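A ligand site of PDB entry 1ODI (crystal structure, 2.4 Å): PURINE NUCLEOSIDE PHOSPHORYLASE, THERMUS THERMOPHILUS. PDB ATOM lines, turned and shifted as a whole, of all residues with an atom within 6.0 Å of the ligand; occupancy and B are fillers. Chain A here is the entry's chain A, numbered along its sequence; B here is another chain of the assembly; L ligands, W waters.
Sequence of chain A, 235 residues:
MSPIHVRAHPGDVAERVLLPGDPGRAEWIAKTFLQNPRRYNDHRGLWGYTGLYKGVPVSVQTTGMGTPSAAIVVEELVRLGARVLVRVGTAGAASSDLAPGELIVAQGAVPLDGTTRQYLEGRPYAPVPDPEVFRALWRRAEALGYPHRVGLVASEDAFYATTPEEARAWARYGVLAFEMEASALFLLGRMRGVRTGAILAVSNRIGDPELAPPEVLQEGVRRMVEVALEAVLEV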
ATOM      1  N   GLY A  21      26.301 -20.739 -15.002  1.00  0.00           N
ATOM      2  CA  GLY A  21      25.360 -19.731 -15.479  1.00  0.00           C
ATOM      3  C   GLY A  21      24.213 -19.496 -14.509  1.00  0.00           C
ATOM      4  O   GLY A  21      23.709 -18.389 -14.370  1.00  0.00           O
ATOM      5  N   GLY A  64      24.922 -15.723 -15.309  1.00  0.00           N
ATOM      6  CA  GLY A  64      23.613 -15.396 -15.841  1.00  0.00           C
ATOM      7  C   GLY A  64      23.581 -16.096 -17.189  1.00  0.00           C
ATOM      8  O   GLY A  64      24.550 -16.782 -17.526  1.00  0.00           O
ATOM      9  N   MET A  65      22.513 -15.940 -17.959  1.00  0.00           N
ATOM     10  CA  MET A  65      22.417 -16.582 -19.261  1.00  0.00           C
ATOM     11  C   MET A  65      22.684 -15.596 -20.402  1.00  0.00           C
ATOM     12  O   MET A  65      22.167 -14.480 -20.407  1.00  0.00           O
ATOM     13  CB  MET A  65      21.022 -17.206 -19.470  1.00  0.00           C
ATOM     14  CG  MET A  65      20.594 -18.177 -18.409  1.00  0.00           C
ATOM     15  SD  MET A  65      19.011 -18.989 -18.793  1.00  0.00           S
ATOM     16  CE  MET A  65      17.837 -17.621 -18.431  1.00  0.00           C
ATOM     17  N   GLY A  66      23.479 -16.031 -21.375  1.00  0.00           N
ATOM     18  CA  GLY A  66      23.756 -15.175 -22.521  1.00  0.00           C
ATOM     19  C   GLY A  66      25.096 -14.481 -22.410  1.00  0.00           C
ATOM     20  O   GLY A  66      25.490 -14.055 -21.323  1.00  0.00           O
ATOM     21  N   ARG A  87      34.324 -21.960 -17.178  1.00  0.00           N
ATOM     22  CA  ARG A  87      32.886 -22.045 -17.196  1.00  0.00           C
ATOM     23  C   ARG A  87      32.445 -23.497 -16.989  1.00  0.00           C
ATOM     24  O   ARG A  87      32.945 -24.408 -17.648  1.00  0.00           O
ATOM     25  CB  ARG A  87      32.357 -21.509 -18.543  1.00  0.00           C
ATOM     26  CG  ARG A  87      30.928 -21.942 -18.911  1.00  0.00           C
ATOM     27  CD  ARG A  87      30.400 -21.218 -20.156  1.00  0.00           C
ATOM     28  NE  ARG A  87      29.256 -21.907 -20.734  1.00  0.00           N
ATOM     29  CZ  ARG A  87      28.119 -22.158 -20.088  1.00  0.00           C
ATOM     30  NH1 ARG A  87      27.959 -21.743 -18.830  1.00  0.00           N
ATOM     31  NH2 ARG A  87      27.147 -22.846 -20.678  1.00  0.00           N
ATOM     32  N   THR A  90      25.854 -26.057 -18.792  1.00  0.00           N
ATOM     33  CA  THR A  90      25.136 -27.154 -19.424  1.00  0.00           C
ATOM     34  C   THR A  90      24.929 -26.755 -20.880  1.00  0.00           C
ATOM     35  O   THR A  90      25.104 -25.595 -21.237  1.00  0.00           O
ATOM     36  CB  THR A  90      23.770 -27.403 -18.750  1.00  0.00           C
ATOM     37  OG1 THR A  90      22.939 -26.246 -18.911  1.00  0.00           O
ATOM     38  CG2 THR A  90      23.954 -27.675 -17.263  1.00  0.00           C
ATOM     39  N   ALA A  91      24.576 -27.717 -21.731  1.00  0.00           N
ATOM     40  CA  ALA A  91      24.353 -27.441 -23.148  1.00  0.00           C
ATOM     41  C   ALA A  91      23.364 -28.421 -23.767  1.00  0.00           C
ATOM     42  O   ALA A  91      23.064 -29.468 -23.196  1.00  0.00           O
ATOM     43  CB  ALA A  91      25.699 -27.487 -23.902  1.00  0.00           C
ATOM     44  N   GLY A  92      22.853 -28.068 -24.952  1.00  0.00           N
ATOM     45  CA  GLY A  92      21.914 -28.920 -25.648  1.00  0.00           C
ATOM     46  C   GLY A  92      22.571 -29.637 -26.800  1.00  0.00           C
ATOM     47  O   GLY A  92      23.131 -28.991 -27.688  1.00  0.00           O
ATOM     48  N   ALA A  93      22.527 -30.979 -26.798  1.00  0.00           N
ATOM     49  CA  ALA A  93      23.144 -31.789 -27.861  1.00  0.00           C
ATOM     50  C   ALA A  93      22.602 -31.476 -29.257  1.00  0.00           C
ATOM     51  O   ALA A  93      21.391 -31.371 -29.470  1.00  0.00           O
ATOM     52  CB  ALA A  93      22.963 -33.255 -27.559  1.00  0.00           C
ATOM     53  N   GLU A 156      25.112 -19.319 -28.833  1.00  0.00           N
ATOM     54  CA  GLU A 156      24.023 -18.611 -29.515  1.00  0.00           C
ATOM     55  C   GLU A 156      23.317 -17.597 -28.617  1.00  0.00           C
ATOM     56  O   GLU A 156      23.527 -17.548 -27.406  1.00  0.00           O
ATOM     57  CB  GLU A 156      22.996 -19.613 -30.027  1.00  0.00           C
ATOM     58  CG  GLU A 156      22.352 -20.443 -28.925  1.00  0.00           C
ATOM     59  CD  GLU A 156      21.194 -21.282 -29.428  1.00  0.00           C
ATOM     60  OE1 GLU A 156      20.604 -22.036 -28.638  1.00  0.00           O
ATOM     61  OE2 GLU A 156      20.874 -21.189 -30.635  1.00  0.00           O
ATOM     62  N   PHE A 159      17.651 -18.832 -27.649  1.00  0.00           N
ATOM     63  CA  PHE A 159      17.376 -20.187 -27.191  1.00  0.00           C
ATOM     64  C   PHE A 159      16.253 -20.826 -27.998  1.00  0.00           C
ATOM     65  O   PHE A 159      16.385 -21.950 -28.465  1.00  0.00           O
ATOM     66  CB  PHE A 159      16.983 -20.176 -25.713  1.00  0.00           C
ATOM     67  CG  PHE A 159      16.831 -21.555 -25.120  1.00  0.00           C
ATOM     68  CD1 PHE A 159      17.917 -22.186 -24.507  1.00  0.00           C
ATOM     69  CD2 PHE A 159      15.606 -22.223 -25.155  1.00  0.00           C
ATOM     70  CE1 PHE A 159      17.784 -23.459 -23.938  1.00  0.00           C
ATOM     71  CE2 PHE A 159      15.460 -23.500 -24.596  1.00  0.00           C
ATOM     72  CZ  PHE A 159      16.562 -24.116 -23.981  1.00  0.00           C
ATOM     73  N   PHE A 178      24.852 -26.778 -28.254  1.00  0.00           N
ATOM     74  CA  PHE A 178      24.612 -25.361 -28.208  1.00  0.00           C
ATOM     75  C   PHE A 178      24.496 -24.886 -26.781  1.00  0.00           C
ATOM     76  O   PHE A 178      23.856 -25.526 -25.952  1.00  0.00           O
ATOM     77  CB  PHE A 178      23.310 -24.991 -28.950  1.00  0.00           C
ATOM     78  CG  PHE A 178      23.413 -25.117 -30.429  1.00  0.00           C
ATOM     79  CD1 PHE A 178      23.429 -26.372 -31.043  1.00  0.00           C
ATOM     80  CD2 PHE A 178      23.539 -23.983 -31.227  1.00  0.00           C
ATOM     81  CE1 PHE A 178      23.580 -26.491 -32.427  1.00  0.00           C
ATOM     82  CE2 PHE A 178      23.694 -24.092 -32.619  1.00  0.00           C
ATOM     83  CZ  PHE A 178      23.711 -25.357 -33.210  1.00  0.00           C
ATOM     84  N   GLU A 179      25.154 -23.766 -26.500  1.00  0.00           N
ATOM     85  CA  GLU A 179      25.120 -23.159 -25.189  1.00  0.00           C
ATOM     86  C   GLU A 179      25.167 -21.640 -25.412  1.00  0.00           C
ATOM     87  O   GLU A 179      25.188 -21.190 -26.567  1.00  0.00           O
ATOM     88  CB  GLU A 179      26.260 -23.679 -24.316  1.00  0.00           C
ATOM     89  CG  GLU A 179      27.618 -23.623 -24.929  1.00  0.00           C
ATOM     90  CD  GLU A 179      28.373 -22.409 -24.473  1.00  0.00           C
ATOM     91  OE1 GLU A 179      28.463 -21.438 -25.255  1.00  0.00           O
ATOM     92  OE2 GLU A 179      28.857 -22.422 -23.323  1.00  0.00           O
ATOM     93  N   MET A 180      25.172 -20.845 -24.339  1.00  0.00           N
ATOM     94  CA  MET A 180      25.123 -19.398 -24.503  1.00  0.00           C
ATOM     95  C   MET A 180      26.127 -18.510 -23.760  1.00  0.00           C
ATOM     96  O   MET A 180      25.780 -17.408 -23.349  1.00  0.00           O
ATOM     97  CB  MET A 180      23.719 -18.911 -24.132  1.00  0.00           C
ATOM     98  CG  MET A 180      22.586 -19.581 -24.913  1.00  0.00           C
ATOM     99  SD  MET A 180      20.936 -19.210 -24.240  1.00  0.00           S
ATOM    100  CE  MET A 180      20.776 -17.464 -24.670  1.00  0.00           C
ATOM    101  N   GLU A 181      27.367 -18.971 -23.579  1.00  0.00           N
ATOM    102  CA  GLU A 181      28.322 -18.126 -22.887  1.00  0.00           C
ATOM    103  C   GLU A 181      29.767 -18.268 -23.326  1.00  0.00           C
ATOM    104  O   GLU A 181      30.526 -17.301 -23.296  1.00  0.00           O
ATOM    105  CB  GLU A 181      28.247 -18.340 -21.373  1.00  0.00           C
ATOM    106  CG  GLU A 181      26.984 -17.821 -20.712  1.00  0.00           C
ATOM    107  CD  GLU A 181      25.892 -18.871 -20.630  1.00  0.00           C
ATOM    108  OE1 GLU A 181      24.693 -18.500 -20.525  1.00  0.00           O
ATOM    109  OE2 GLU A 181      26.237 -20.068 -20.676  1.00  0.00           O
ATOM    110  N   LEU A 200      31.223 -28.581 -20.135  1.00  0.00           N
ATOM    111  CA  LEU A 200      29.775 -28.645 -20.107  1.00  0.00           C
ATOM    112  C   LEU A 200      29.190 -30.016 -19.847  1.00  0.00           C
ATOM    113  O   LEU A 200      29.811 -31.039 -20.147  1.00  0.00           O
ATOM    114  CB  LEU A 200      29.245 -28.112 -21.425  1.00  0.00           C
ATOM    115  CG  LEU A 200      29.881 -26.774 -21.807  1.00  0.00           C
ATOM    116  CD1 LEU A 200      30.170 -26.750 -23.294  1.00  0.00           C
ATOM    117  CD2 LEU A 200      28.957 -25.652 -21.403  1.00  0.00           C
ATOM    118  N   SER A 203      22.494 -31.331 -20.843  1.00  0.00           N
ATOM    119  CA  SER A 203      21.290 -31.426 -20.021  1.00  0.00           C
ATOM    120  C   SER A 203      20.046 -31.735 -20.843  1.00  0.00           C
ATOM    121  O   SER A 203      18.970 -32.007 -20.301  1.00  0.00           O
ATOM    122  CB  SER A 203      21.085 -30.135 -19.231  1.00  0.00           C
ATOM    123  OG  SER A 203      21.050 -29.020 -20.092  1.00  0.00           O
ATOM    124  N   ASN A 204      20.196 -31.703 -22.158  1.00  0.00           N
ATOM    125  CA  ASN A 204      19.079 -31.964 -23.054  1.00  0.00           C
ATOM    126  C   ASN A 204      19.506 -32.031 -24.517  1.00  0.00           C
ATOM    127  O   ASN A 204      20.610 -31.628 -24.888  1.00  0.00           O
ATOM    128  CB  ASN A 204      18.042 -30.863 -22.904  1.00  0.00           C
ATOM    129  CG  ASN A 204      18.545 -29.530 -23.425  1.00  0.00           C
ATOM    130  OD1 ASN A 204      18.307 -29.169 -24.584  1.00  0.00           O
ATOM    131  ND2 ASN A 204      19.259 -28.790 -22.587  1.00  0.00           N
ATOM    132  N   ARG A 205      18.619 -32.566 -25.335  1.00  0.00           N
ATOM    133  CA  ARG A 205      18.855 -32.630 -26.767  1.00  0.00           C
ATOM    134  C   ARG A 205      18.037 -31.450 -27.307  1.00  0.00           C
ATOM    135  O   ARG A 205      16.956 -31.158 -26.792  1.00  0.00           O
ATOM    136  CB  ARG A 205      18.353 -33.974 -27.349  1.00  0.00           C
ATOM    137  CG  ARG A 205      19.061 -35.190 -26.769  1.00  0.00           C
ATOM    138  CD  ARG A 205      18.815 -36.433 -27.610  1.00  0.00           C
ATOM    139  NE  ARG A 205      19.632 -37.569 -27.189  1.00  0.00           N
ATOM    140  CZ  ARG A 205      19.363 -38.377 -26.165  1.00  0.00           C
ATOM    141  NH1 ARG A 205      18.267 -38.171 -25.429  1.00  0.00           N
ATOM    142  NH2 ARG A 205      20.166 -39.393 -25.892  1.00  0.00           N
ATOM    143  N   ILE A 206      18.557 -30.742 -28.296  1.00  0.00           N
ATOM    144  CA  ILE A 206      17.852 -29.593 -28.829  1.00  0.00           C
ATOM    145  C   ILE A 206      16.442 -29.936 -29.286  1.00  0.00           C
ATOM    146  O   ILE A 206      16.240 -30.861 -30.078  1.00  0.00           O
ATOM    147  CB  ILE A 206      18.634 -28.956 -30.007  1.00  0.00           C
ATOM    148  CG1 ILE A 206      19.881 -28.243 -29.473  1.00  0.00           C
ATOM    149  CG2 ILE A 206      17.734 -27.986 -30.766  1.00  0.00           C
ATOM    150  CD1 ILE A 206      19.670 -26.796 -29.047  1.00  0.00           C
ATOM    151  N   GLY A 207      15.465 -29.185 -28.781  1.00  0.00           N
ATOM    152  CA  GLY A 207      14.081 -29.413 -29.146  1.00  0.00           C
ATOM    153  C   GLY A 207      13.255 -30.063 -28.058  1.00  0.00           C
ATOM    154  O   GLY A 207      12.034 -30.155 -28.181  1.00  0.00           O
ATOM    155  N   LEU A 211      14.106 -30.532 -19.496  1.00  0.00           N
ATOM    156  CA  LEU A 211      15.479 -31.004 -19.322  1.00  0.00           C
ATOM    157  C   LEU A 211      15.423 -32.451 -18.842  1.00  0.00           C
ATOM    158  O   LEU A 211      14.344 -32.955 -18.527  1.00  0.00           O
ATOM    159  CB  LEU A 211      16.216 -30.138 -18.298  1.00  0.00           C
ATOM    160  CG  LEU A 211      16.317 -28.629 -18.557  1.00  0.00           C
ATOM    161  CD1 LEU A 211      17.068 -27.965 -17.419  1.00  0.00           C
ATOM    162  CD2 LEU A 211      17.011 -28.377 -19.894  1.00  0.00           C
ATOM    163  N   ILE B   4      11.083 -24.293 -19.193  1.00  0.00           N
ATOM    164  CA  ILE B   4      12.435 -24.648 -18.804  1.00  0.00           C
ATOM    165  C   ILE B   4      13.098 -23.687 -17.821  1.00  0.00           C
ATOM    166  O   ILE B   4      13.833 -24.126 -16.939  1.00  0.00           O
ATOM    167  CB  ILE B   4      13.323 -24.817 -20.049  1.00  0.00           C
ATOM    168  CG1 ILE B   4      12.794 -25.972 -20.894  1.00  0.00           C
ATOM    169  CG2 ILE B   4      14.763 -25.065 -19.645  1.00  0.00           C
ATOM    170  CD1 ILE B   4      13.679 -26.374 -22.056  1.00  0.00           C
ATOM    171  N   HIS B   5      12.847 -22.392 -17.951  1.00  0.00           N
ATOM    172  CA  HIS B   5      13.485 -21.417 -17.064  1.00  0.00           C
ATOM    173  C   HIS B   5      12.567 -20.764 -16.034  1.00  0.00           C
ATOM    174  O   HIS B   5      12.871 -20.769 -14.841  1.00  0.00           O
ATOM    175  CB  HIS B   5      14.203 -20.356 -17.901  1.00  0.00           C
ATOM    176  CG  HIS B   5      15.063 -20.930 -18.983  1.00  0.00           C
ATOM    177  ND1 HIS B   5      14.538 -21.579 -20.083  1.00  0.00           N
ATOM    178  CD2 HIS B   5      16.404 -20.972 -19.125  1.00  0.00           C
ATOM    179  CE1 HIS B   5      15.534 -21.990 -20.857  1.00  0.00           C
ATOM    180  NE2 HIS B   5      16.675 -21.634 -20.295  1.00  0.00           N
ATOM    181  N   ARG B  44      16.901 -20.078 -11.225  1.00  0.00           N
ATOM    182  CA  ARG B  44      17.877 -19.277 -11.978  1.00  0.00           C
ATOM    183  C   ARG B  44      17.868 -17.802 -11.610  1.00  0.00           C
ATOM    184  O   ARG B  44      18.274 -16.949 -12.410  1.00  0.00           O
ATOM    185  CB  ARG B  44      17.665 -19.447 -13.486  1.00  0.00           C
ATOM    186  CG  ARG B  44      18.326 -20.689 -14.083  1.00  0.00           C
ATOM    187  CD  ARG B  44      18.187 -20.694 -15.602  1.00  0.00           C
ATOM    188  NE  ARG B  44      18.793 -21.857 -16.238  1.00  0.00           N
ATOM    189  CZ  ARG B  44      20.096 -21.974 -16.521  1.00  0.00           C
ATOM    190  NH1 ARG B  44      20.951 -21.005 -16.209  1.00  0.00           N
ATOM    191  NH2 ARG B  44      20.542 -23.068 -17.136  1.00  0.00           N
ATOM    192  N   ILE B  72      14.318 -15.349 -23.578  1.00  0.00           N
ATOM    193  CA  ILE B  72      13.890 -16.599 -22.970  1.00  0.00           C
ATOM    194  C   ILE B  72      12.697 -16.363 -22.076  1.00  0.00           C
ATOM    195  O   ILE B  72      11.675 -17.040 -22.189  1.00  0.00           O
ATOM    196  CB  ILE B  72      15.028 -17.240 -22.166  1.00  0.00           C
ATOM    197  CG1 ILE B  72      15.959 -18.007 -23.121  1.00  0.00           C
ATOM    198  CG2 ILE B  72      14.462 -18.164 -21.090  1.00  0.00           C
ATOM    199  CD1 ILE B  72      17.166 -18.615 -22.455  1.00  0.00           C
HETATM  200  O1  LIG L   1      18.961 -23.104 -20.262  1.00  0.00           O
HETATM  201  C1  LIG L   1      19.726 -22.328 -21.175  1.00  0.00           C
HETATM  202  C2  LIG L   1      21.079 -22.112 -20.469  1.00  0.00           C
HETATM  203  O2  LIG L   1      21.822 -23.359 -20.178  1.00  0.00           O
HETATM  204  C3  LIG L   1      22.042 -21.292 -21.308  1.00  0.00           C
HETATM  205  O3  LIG L   1      22.684 -20.381 -20.405  1.00  0.00           O
HETATM  206  C4  LIG L   1      23.037 -22.300 -21.934  1.00  0.00           C
HETATM  207  O4  LIG L   1      24.410 -21.965 -21.731  1.00  0.00           O
HETATM  208  C5  LIG L   1      22.584 -23.677 -21.367  1.00  0.00           C
HETATM  209  N1  LIG L   1      21.796 -24.561 -22.318  1.00  0.00           N
HETATM  210  C6  LIG L   1      21.313 -25.841 -21.988  1.00  0.00           C
HETATM  211  N2  LIG L   1      20.650 -26.455 -22.940  1.00  0.00           N
HETATM  212  C7  LIG L   1      20.682 -25.532 -23.997  1.00  0.00           C
HETATM  213  C8  LIG L   1      20.128 -25.565 -25.347  1.00  0.00           C
HETATM  214  N3  LIG L   1      19.435 -26.602 -25.826  1.00  0.00           N
HETATM  215  N4  LIG L   1      20.354 -24.461 -26.142  1.00  0.00           N
HETATM  216  C9  LIG L   1      21.048 -23.400 -25.656  1.00  0.00           C
HETATM  217  N5  LIG L   1      21.605 -23.259 -24.414  1.00  0.00           N
HETATM  218  C10 LIG L   1      21.384 -24.359 -23.635  1.00  0.00           C
HETATM  219  O   HOH W   1      18.855 -23.902 -28.408  1.00  0.00           O
HETATM  220  O   HOH W   2      18.627 -25.000 -18.430  1.00  0.00           O
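A nitrogen (N4) of the ligand sits close to the side-chain carboxylate (OE1) of Glu 156 (3.5 Å).
Merely in contact with the ligand: Ile 206 (3.2 Å), Phe 159 (3.5 Å), Ala 91 (3.5 Å), Phe 178 (3.5 Å), Glu 179 (3.6 Å), Met 65 (3.6 Å) and Ser 203 (3.7 Å).
Hydrophobic or aromatic side chains that line the ligand: Met 65, Phe 159, Met 180, Ile 206 and His 5 of chain B.
16 residues have an atom within 4 Å of the ligand: Met 65, Arg 87, Thr 90, Ala 91, Gly 92, Glu 156, Phe 159, Phe 178, Glu 179, Met 180, Glu 181, Ser 203, Asn 204, Ile 206, His 5 of chain B and Arg 44 of chain B.
Water W2 lies within hydrogen-bond range of O1 of the ligand (2.7 Å) and NH2 of Arg 44 of chain B (3.0 Å).
The side-chain amide nitrogen (ND2) of Asn 204 lies within hydrogen-bond range of the side-chain hydroxyl (OG) of Ser 203, 3.1 Å away.
O of Asn 204 sits at hydrogen-bond distance from N of Ala 93, 2.8 Å away.
The backbone carbonyl oxygen (O) of Met 180 sits close to the backbone NH (N) of Gly 66 (3.3 Å).
The backbone carbonyl oxygen (O) of Thr 90 is in hydrogen-bond range of the guanidinium group (NH2) of Arg 87 (3.5 Å).
The side-chain carboxylate (OE2) of Glu 179 is in salt-bridge range of the guanidinium group (NE) of Arg 87 (2.7 Å).
The backbone NH (N) of Ile 206 lies within hydrogen-bond range of the backbone carbonyl oxygen (O) of Ala 93 (3.1 Å).
The backbone NH (N) of Glu 156 is in hydrogen-bond range of the backbone carbonyl oxygen (O) of Glu 179 (2.9 Å).
The backbone carbonyl oxygen (O) of Gly 92 is in hydrogen-bond range of the backbone NH (N) of Phe 178 (2.9 Å).
An oxygen (O1) of the ligand lies within hydrogen-bond range of a ring nitrogen (NE2) of His 5 of chain B, at 2.7 Å.
N2 of the ligand is in hydrogen-bond range of ND2 of Asn 204 (2.7 Å).
An oxygen (O3) of the ligand sits at hydrogen-bond distance from the side-chain carboxylate of Glu 181 (2.8 Å).
O4 of the ligand is in hydrogen-bond range of N of Met 180, 2.9 Å away.
The guanidinium group (NH2) of Arg 87 sits at hydrogen-bond distance from an oxygen (O4) of the ligand (3.1 Å).
The side-chain hydroxyl of Thr 90 lies within hydrogen-bond range of an oxygen (O2) of the ligand, at 3.3 Å.
The guanidinium group (NH2) of Arg 44 of chain B is in hydrogen-bond range of an oxygen (O2) of the ligand, at 3.3 Å.
The backbone NH (N) of Gly 92 is in hydrogen-bond range of a nitrogen (N2) of the ligand, 3.4 Å away.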
